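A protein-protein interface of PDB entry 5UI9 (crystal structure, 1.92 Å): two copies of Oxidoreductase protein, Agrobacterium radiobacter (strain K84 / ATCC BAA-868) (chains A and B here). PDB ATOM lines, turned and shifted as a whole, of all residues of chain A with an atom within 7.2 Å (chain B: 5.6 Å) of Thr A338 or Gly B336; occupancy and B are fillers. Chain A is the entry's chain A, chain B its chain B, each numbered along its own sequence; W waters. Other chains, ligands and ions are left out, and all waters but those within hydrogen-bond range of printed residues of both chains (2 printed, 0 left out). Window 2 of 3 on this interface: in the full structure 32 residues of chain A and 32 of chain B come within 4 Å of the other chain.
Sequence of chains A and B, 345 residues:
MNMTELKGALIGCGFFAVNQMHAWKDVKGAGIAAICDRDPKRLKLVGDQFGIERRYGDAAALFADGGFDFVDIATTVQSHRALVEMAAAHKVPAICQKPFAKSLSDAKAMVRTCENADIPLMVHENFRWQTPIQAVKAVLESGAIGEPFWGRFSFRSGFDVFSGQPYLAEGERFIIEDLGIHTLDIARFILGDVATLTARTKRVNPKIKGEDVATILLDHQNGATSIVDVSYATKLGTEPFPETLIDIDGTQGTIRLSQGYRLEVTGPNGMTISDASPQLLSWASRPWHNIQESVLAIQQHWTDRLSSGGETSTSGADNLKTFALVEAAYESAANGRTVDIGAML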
ATOM      1  N   ALA A 195      -2.207 -19.919 -38.493  1.00  0.00           N
ATOM      2  CA  ALA A 195      -3.142 -20.757 -37.735  1.00  0.00           C
ATOM      3  C   ALA A 195      -4.064 -19.906 -36.877  1.00  0.00           C
ATOM      4  O   ALA A 195      -5.287 -20.053 -36.934  1.00  0.00           O
ATOM      5  CB  ALA A 195      -2.381 -21.741 -36.854  1.00  0.00           C
ATOM      6  N   THR A 196      -3.464 -19.030 -36.069  1.00  0.00           N
ATOM      7  CA  THR A 196      -4.209 -18.159 -35.152  1.00  0.00           C
ATOM      8  C   THR A 196      -3.654 -16.738 -35.183  1.00  0.00           C
ATOM      9  O   THR A 196      -2.507 -16.508 -35.576  1.00  0.00           O
ATOM     10  CB  THR A 196      -4.207 -18.691 -33.700  1.00  0.00           C
ATOM     11  OG1 THR A 196      -2.863 -18.904 -33.266  1.00  0.00           O
ATOM     12  CG2 THR A 196      -4.964 -20.005 -33.590  1.00  0.00           C
ATOM     13  N   LEU A 197      -4.492 -15.801 -34.752  1.00  0.00           N
ATOM     14  CA  LEU A 197      -4.246 -14.373 -34.919  1.00  0.00           C
ATOM     15  C   LEU A 197      -4.897 -13.573 -33.785  1.00  0.00           C
ATOM     16  O   LEU A 197      -6.007 -13.890 -33.360  1.00  0.00           O
ATOM     17  CB  LEU A 197      -4.819 -13.954 -36.276  1.00  0.00           C
ATOM     18  CG  LEU A 197      -4.705 -12.507 -36.748  1.00  0.00           C
ATOM     19  CD1 LEU A 197      -4.604 -12.425 -38.266  1.00  0.00           C
ATOM     20  CD2 LEU A 197      -5.863 -11.647 -36.252  1.00  0.00           C
ATOM     21  N   THR A 198      -4.196 -12.545 -33.307  1.00  0.00           N
ATOM     22  CA  THR A 198      -4.720 -11.608 -32.306  1.00  0.00           C
ATOM     23  C   THR A 198      -4.367 -10.183 -32.718  1.00  0.00           C
ATOM     24  O   THR A 198      -3.223  -9.918 -33.082  1.00  0.00           O
ATOM     25  CB  THR A 198      -4.110 -11.853 -30.909  1.00  0.00           C
ATOM     26  OG1 THR A 198      -3.847 -13.249 -30.732  1.00  0.00           O
ATOM     27  CG2 THR A 198      -5.049 -11.374 -29.819  1.00  0.00           C
ATOM     28  N   ALA A 199      -5.335  -9.271 -32.652  1.00  0.00           N
ATOM     29  CA  ALA A 199      -5.153  -7.911 -33.163  1.00  0.00           C
ATOM     30  C   ALA A 199      -5.656  -6.842 -32.201  1.00  0.00           C
ATOM     31  O   ALA A 199      -6.525  -7.096 -31.367  1.00  0.00           O
ATOM     32  CB  ALA A 199      -5.828  -7.762 -34.513  1.00  0.00           C
ATOM     33  N   ARG A 200      -5.072  -5.652 -32.329  1.00  0.00           N
ATOM     34  CA  ARG A 200      -5.459  -4.460 -31.578  1.00  0.00           C
ATOM     35  C   ARG A 200      -5.450  -3.284 -32.536  1.00  0.00           C
ATOM     36  O   ARG A 200      -4.548  -3.176 -33.364  1.00  0.00           O
ATOM     37  CB  ARG A 200      -4.467  -4.182 -30.445  1.00  0.00           C
ATOM     38  CG  ARG A 200      -4.316  -5.311 -29.449  1.00  0.00           C
ATOM     39  CD  ARG A 200      -5.579  -5.500 -28.636  1.00  0.00           C
ATOM     40  NE  ARG A 200      -5.386  -6.514 -27.600  1.00  0.00           N
ATOM     41  CZ  ARG A 200      -5.619  -7.817 -27.734  1.00  0.00           C
ATOM     42  NH1 ARG A 200      -6.122  -8.335 -28.853  1.00  0.00           N
ATOM     43  NH2 ARG A 200      -5.369  -8.617 -26.706  1.00  0.00           N
ATOM     44  N   LEU A 217      -0.560 -10.025 -33.838  1.00  0.00           N
ATOM     45  CA  LEU A 217       0.344 -11.119 -33.475  1.00  0.00           C
ATOM     46  C   LEU A 217      -0.084 -12.387 -34.216  1.00  0.00           C
ATOM     47  O   LEU A 217      -1.210 -12.844 -34.044  1.00  0.00           O
ATOM     48  CB  LEU A 217       0.286 -11.355 -31.968  1.00  0.00           C
ATOM     49  CG  LEU A 217       1.125 -12.464 -31.330  1.00  0.00           C
ATOM     50  CD1 LEU A 217       2.614 -12.281 -31.563  1.00  0.00           C
ATOM     51  CD2 LEU A 217       0.835 -12.500 -29.833  1.00  0.00           C
ATOM     52  N   ASP A 219       0.433 -16.479 -35.255  1.00  0.00           N
ATOM     53  CA  ASP A 219       0.989 -17.805 -35.005  1.00  0.00           C
ATOM     54  C   ASP A 219       0.921 -18.570 -36.325  1.00  0.00           C
ATOM     55  O   ASP A 219      -0.161 -18.957 -36.762  1.00  0.00           O
ATOM     56  CB  ASP A 219       0.198 -18.497 -33.904  1.00  0.00           C
ATOM     57  CG  ASP A 219       0.052 -17.620 -32.657  1.00  0.00           C
ATOM     58  OD1 ASP A 219       1.091 -17.219 -32.084  1.00  0.00           O
ATOM     59  OD2 ASP A 219      -1.092 -17.323 -32.241  1.00  0.00           O
ATOM     60  N   ALA A 328     -10.339 -11.632 -39.668  1.00  0.00           N
ATOM     61  CA  ALA A 328      -9.983 -12.115 -38.335  1.00  0.00           C
ATOM     62  C   ALA A 328      -9.404 -11.013 -37.443  1.00  0.00           C
ATOM     63  O   ALA A 328      -9.666 -10.994 -36.245  1.00  0.00           O
ATOM     64  CB  ALA A 328      -9.002 -13.271 -38.436  1.00  0.00           C
ATOM     65  N   GLU A 331     -12.333  -8.792 -36.275  1.00  0.00           N
ATOM     66  CA  GLU A 331     -13.023  -9.599 -35.260  1.00  0.00           C
ATOM     67  C   GLU A 331     -12.272  -9.560 -33.929  1.00  0.00           C
ATOM     68  O   GLU A 331     -12.845  -9.193 -32.904  1.00  0.00           O
ATOM     69  CB  GLU A 331     -13.181 -11.046 -35.738  1.00  0.00           C
ATOM     70  CG  GLU A 331     -14.029 -11.937 -34.838  1.00  0.00           C
ATOM     71  CD  GLU A 331     -14.214 -13.350 -35.388  1.00  0.00           C
ATOM     72  OE1 GLU A 331     -14.187 -13.545 -36.630  1.00  0.00           O
ATOM     73  OE2 GLU A 331     -14.388 -14.278 -34.565  1.00  0.00           O
ATOM     74  N   SER A 332     -10.987  -9.913 -33.967  1.00  0.00           N
ATOM     75  CA  SER A 332     -10.143  -9.965 -32.767  1.00  0.00           C
ATOM     76  C   SER A 332     -10.039  -8.628 -32.042  1.00  0.00           C
ATOM     77  O   SER A 332     -10.078  -8.591 -30.813  1.00  0.00           O
ATOM     78  CB  SER A 332      -8.733 -10.449 -33.115  1.00  0.00           C
ATOM     79  OG  SER A 332      -7.909 -10.477 -31.962  1.00  0.00           O
ATOM     80  N   ASN A 335     -13.514  -8.035 -30.178  1.00  0.00           N
ATOM     81  CA  ASN A 335     -13.773  -9.003 -29.090  1.00  0.00           C
ATOM     82  C   ASN A 335     -12.636  -9.109 -28.071  1.00  0.00           C
ATOM     83  O   ASN A 335     -12.860  -9.540 -26.941  1.00  0.00           O
ATOM     84  CB  ASN A 335     -14.014 -10.409 -29.668  1.00  0.00           C
ATOM     85  CG  ASN A 335     -15.180 -10.459 -30.647  1.00  0.00           C
ATOM     86  OD1 ASN A 335     -16.234  -9.860 -30.417  1.00  0.00           O
ATOM     87  ND2 ASN A 335     -14.996 -11.186 -31.747  1.00  0.00           N
ATOM     88  N   GLY A 336     -11.420  -8.749 -28.482  1.00  0.00           N
ATOM     89  CA  GLY A 336     -10.223  -8.941 -27.665  1.00  0.00           C
ATOM     90  C   GLY A 336      -9.728 -10.378 -27.629  1.00  0.00           C
ATOM     91  O   GLY A 336      -8.808 -10.687 -26.871  1.00  0.00           O
ATOM     92  N   ARG A 337     -10.301 -11.242 -28.474  1.00  0.00           N
ATOM     93  CA  ARG A 337     -10.043 -12.681 -28.448  1.00  0.00           C
ATOM     94  C   ARG A 337      -9.135 -13.114 -29.613  1.00  0.00           C
ATOM     95  O   ARG A 337      -9.100 -12.473 -30.668  1.00  0.00           O
ATOM     96  CB  ARG A 337     -11.375 -13.440 -28.502  1.00  0.00           C
ATOM     97  N   THR A 338      -8.396 -14.201 -29.401  1.00  0.00           N
ATOM     98  CA  THR A 338      -7.629 -14.849 -30.461  1.00  0.00           C
ATOM     99  C   THR A 338      -8.602 -15.555 -31.412  1.00  0.00           C
ATOM    100  O   THR A 338      -9.607 -16.113 -30.970  1.00  0.00           O
ATOM    101  CB  THR A 338      -6.617 -15.855 -29.873  1.00  0.00           C
ATOM    102  OG1 THR A 338      -5.753 -15.175 -28.953  1.00  0.00           O
ATOM    103  CG2 THR A 338      -5.767 -16.510 -30.968  1.00  0.00           C
ATOM    104  N   VAL A 339      -8.304 -15.519 -32.709  1.00  0.00           N
ATOM    105  CA  VAL A 339      -9.191 -16.074 -33.736  1.00  0.00           C
ATOM    106  C   VAL A 339      -8.488 -17.214 -34.472  1.00  0.00           C
ATOM    107  O   VAL A 339      -7.342 -17.069 -34.889  1.00  0.00           O
ATOM    108  CB  VAL A 339      -9.643 -14.988 -34.741  1.00  0.00           C
ATOM    109  CG1 VAL A 339     -10.485 -15.587 -35.863  1.00  0.00           C
ATOM    110  CG2 VAL A 339     -10.426 -13.899 -34.024  1.00  0.00           C
ATOM    111  N   ASP A 340      -9.202 -18.330 -34.633  1.00  0.00           N
ATOM    112  CA  ASP A 340      -8.732 -19.479 -35.406  1.00  0.00           C
ATOM    113  C   ASP A 340      -8.975 -19.209 -36.892  1.00  0.00           C
ATOM    114  O   ASP A 340     -10.120 -19.045 -37.320  1.00  0.00           O
ATOM    115  CB  ASP A 340      -9.485 -20.744 -34.962  1.00  0.00           C
ATOM    116  CG  ASP A 340      -8.947 -22.027 -35.600  1.00  0.00           C
ATOM    117  OD1 ASP A 340      -8.483 -22.008 -36.762  1.00  0.00           O
ATOM    118  OD2 ASP A 340      -9.019 -23.078 -34.932  1.00  0.00           O
ATOM    119  N   THR B 198      -0.913 -10.752 -23.797  1.00  0.00           N
ATOM    120  CA  THR B 198      -0.931 -11.990 -24.600  1.00  0.00           C
ATOM    121  C   THR B 198       0.512 -12.354 -24.935  1.00  0.00           C
ATOM    122  O   THR B 198       1.286 -11.474 -25.290  1.00  0.00           O
ATOM    123  CB  THR B 198      -1.706 -11.811 -25.925  1.00  0.00           C
ATOM    124  OG1 THR B 198      -2.952 -11.153 -25.675  1.00  0.00           O
ATOM    125  CG2 THR B 198      -1.987 -13.145 -26.575  1.00  0.00           C
ATOM    126  N   ARG B 200       3.533 -15.484 -26.510  1.00  0.00           N
ATOM    127  CA  ARG B 200       3.933 -16.711 -27.198  1.00  0.00           C
ATOM    128  C   ARG B 200       5.379 -17.006 -26.838  1.00  0.00           C
ATOM    129  O   ARG B 200       6.154 -16.085 -26.597  1.00  0.00           O
ATOM    130  CB  ARG B 200       3.800 -16.551 -28.711  1.00  0.00           C
ATOM    131  CG  ARG B 200       2.400 -16.193 -29.178  1.00  0.00           C
ATOM    132  CD  ARG B 200       1.431 -17.343 -28.975  1.00  0.00           C
ATOM    133  NE  ARG B 200       0.104 -17.004 -29.484  1.00  0.00           N
ATOM    134  CZ  ARG B 200      -0.861 -16.395 -28.796  1.00  0.00           C
ATOM    135  NH1 ARG B 200      -0.711 -16.065 -27.515  1.00  0.00           N
ATOM    136  NH2 ARG B 200      -2.014 -16.132 -29.401  1.00  0.00           N
ATOM    137  N   GLU B 331       1.422 -18.002 -18.315  1.00  0.00           N
ATOM    138  CA  GLU B 331       0.041 -18.492 -18.378  1.00  0.00           C
ATOM    139  C   GLU B 331      -0.507 -18.369 -19.801  1.00  0.00           C
ATOM    140  O   GLU B 331      -1.050 -19.331 -20.343  1.00  0.00           O
ATOM    141  CB  GLU B 331      -0.860 -17.733 -17.397  1.00  0.00           C
ATOM    142  CG  GLU B 331      -2.230 -18.366 -17.182  1.00  0.00           C
ATOM    143  CD  GLU B 331      -3.198 -17.444 -16.454  1.00  0.00           C
ATOM    144  OE1 GLU B 331      -2.781 -16.773 -15.478  1.00  0.00           O
ATOM    145  OE2 GLU B 331      -4.383 -17.392 -16.856  1.00  0.00           O
ATOM    146  N   SER B 332      -0.342 -17.188 -20.396  1.00  0.00           N
ATOM    147  CA  SER B 332      -0.816 -16.912 -21.755  1.00  0.00           C
ATOM    148  C   SER B 332      -0.178 -17.819 -22.803  1.00  0.00           C
ATOM    149  O   SER B 332      -0.871 -18.335 -23.670  1.00  0.00           O
ATOM    150  CB  SER B 332      -0.547 -15.451 -22.125  1.00  0.00           C
ATOM    151  OG  SER B 332      -0.995 -15.174 -23.436  1.00  0.00           O
ATOM    152  N   ALA B 333       1.137 -18.006 -22.711  1.00  0.00           N
ATOM    153  CA  ALA B 333       1.885 -18.858 -23.643  1.00  0.00           C
ATOM    154  C   ALA B 333       1.451 -20.318 -23.614  1.00  0.00           C
ATOM    155  O   ALA B 333       1.458 -20.976 -24.648  1.00  0.00           O
ATOM    156  CB  ALA B 333       3.382 -18.759 -23.364  1.00  0.00           C
ATOM    157  N   ALA B 334       1.085 -20.812 -22.431  1.00  0.00           N
ATOM    158  CA  ALA B 334       0.620 -22.197 -22.250  1.00  0.00           C
ATOM    159  C   ALA B 334      -0.854 -22.381 -22.648  1.00  0.00           C
ATOM    160  O   ALA B 334      -1.193 -23.316 -23.373  1.00  0.00           O
ATOM    161  CB  ALA B 334       0.836 -22.635 -20.806  1.00  0.00           C
ATOM    162  N   ASN B 335      -1.716 -21.490 -22.157  1.00  0.00           N
ATOM    163  CA  ASN B 335      -3.159 -21.535 -22.435  1.00  0.00           C
ATOM    164  C   ASN B 335      -3.502 -21.072 -23.849  1.00  0.00           C
ATOM    165  O   ASN B 335      -4.462 -21.553 -24.430  1.00  0.00           O
ATOM    166  CB  ASN B 335      -3.934 -20.677 -21.421  1.00  0.00           C
ATOM    167  N   GLY B 336      -2.718 -20.143 -24.392  1.00  0.00           N
ATOM    168  CA  GLY B 336      -3.004 -19.516 -25.688  1.00  0.00           C
ATOM    169  C   GLY B 336      -3.896 -18.282 -25.605  1.00  0.00           C
ATOM    170  O   GLY B 336      -4.185 -17.667 -26.634  1.00  0.00           O
ATOM    171  N   ARG B 337      -4.294 -17.896 -24.386  1.00  0.00           N
ATOM    172  CA  ARG B 337      -5.317 -16.870 -24.164  1.00  0.00           C
ATOM    173  C   ARG B 337      -4.741 -15.535 -23.671  1.00  0.00           C
ATOM    174  O   ARG B 337      -3.610 -15.468 -23.178  1.00  0.00           O
ATOM    175  CB  ARG B 337      -6.339 -17.389 -23.147  1.00  0.00           C
ATOM    176  N   THR B 338      -5.542 -14.480 -23.809  1.00  0.00           N
ATOM    177  CA  THR B 338      -5.236 -13.168 -23.239  1.00  0.00           C
ATOM    178  C   THR B 338      -5.508 -13.198 -21.731  1.00  0.00           C
ATOM    179  O   THR B 338      -6.517 -13.749 -21.296  1.00  0.00           O
ATOM    180  CB  THR B 338      -6.076 -12.064 -23.916  1.00  0.00           C
ATOM    181  OG1 THR B 338      -5.826 -12.080 -25.328  1.00  0.00           O
ATOM    182  CG2 THR B 338      -5.727 -10.677 -23.374  1.00  0.00           C
HETATM  183  O   HOH W   1      -2.709  -8.248 -24.898  1.00  0.00           O
HETATM  184  O   HOH W   2      -2.122 -14.867 -32.463  1.00  0.00           O
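The side-chain carboxylate (OD1) of Asp A219 lies within salt-bridge range of the guanidinium group (NE) of Arg B200, at 2.8 Å.
The backbone carbonyl oxygen (O) of Asp A219 sits at hydrogen-bond distance from the backbone NH (N) of Ala A195, at 2.8 Å.
The side-chain hydroxyl (OG1) of Thr A196 sits at hydrogen-bond distance from the side-chain carboxylate (OD2) of Asp A219 (2.6 Å).
The backbone carbonyl oxygen (O) of Thr A198 sits at hydrogen-bond distance from the backbone NH (N) of Leu A217, 2.8 Å away.
The side-chain hydroxyl (OG1) of Thr A338 sits at hydrogen-bond distance from the side-chain hydroxyl (OG1) of Thr A198 (3.2 Å).
The side-chain hydroxyl (OG1) of Thr B198 is in hydrogen-bond range of the side-chain hydroxyl (OG1) of Thr B338, 3.0 Å away.
Among the printed residues, merely in contact across the chains: Gly A336 with Thr B338, Arg A200 with Thr B198, Thr A198 with Arg B200, Thr A338 with Gly B336, Arg A200 with Thr B338 and Thr A338 with Arg B200.
Of the printed residues of chain B, Asp A219 touches Arg B200.
Of chain B, only Arg B200 (3.9 Å) and Gly B336 (3.7 Å) come within 4 Å of Thr A338.
Of the printed residues of chain A, Arg B200 touches Thr A198 (3.7 Å), Asp A219 (2.8 Å) and Thr A338 (3.9 Å).
Gly B336 touches one residue of chain A.
Printed residues of chain A within 4 Å of Thr B338: Arg A200 (3.8 Å) and Gly A336 (3.6 Å).
The nearest printed residue of chain B that does not touch Arg A200 is Arg B337 (7.6 Å).
Of the 17 printed residues of chain A, 5 touch a printed residue of chain B.
Printed residues of chain A that touch a printed residue of chain B: Thr A198, Arg A200, Asp A219, Gly A336 and Thr A338.
Among the printed residues, 7 pairs touch across the chains.
Among the printed residues, Asp or Glu carboxylates within 4 Å of a Lys or Arg side-chain nitrogen of the other chain: Asp A219 with Arg B200.
Thr A198 touches Arg B200, and with the chains exchanged Arg A200 touches Thr B198.
Arg A200 touches Thr B338, and with the chains exchanged Thr A338 touches Arg B200.
Gly A336 touches Thr B338, and with the chains exchanged Thr A338 touches Gly B336.
Positions printed for both chains: 198, 200, 331, 332, 335, 336, 337 and 338.
Water W2 lies within hydrogen-bond range of OD2 of Asp A219 (2.7 Å), O of Leu A217 (2.7 Å), OG1 of Thr A198 (2.9 Å), NH2 of Arg B200 (3.3 Å) and N of Leu A197 (3.4 Å).
Water W1 lies within hydrogen-bond range of OG1 of Thr B198 (3.0 Å) and NH2 of Arg A200 (3.2 Å).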
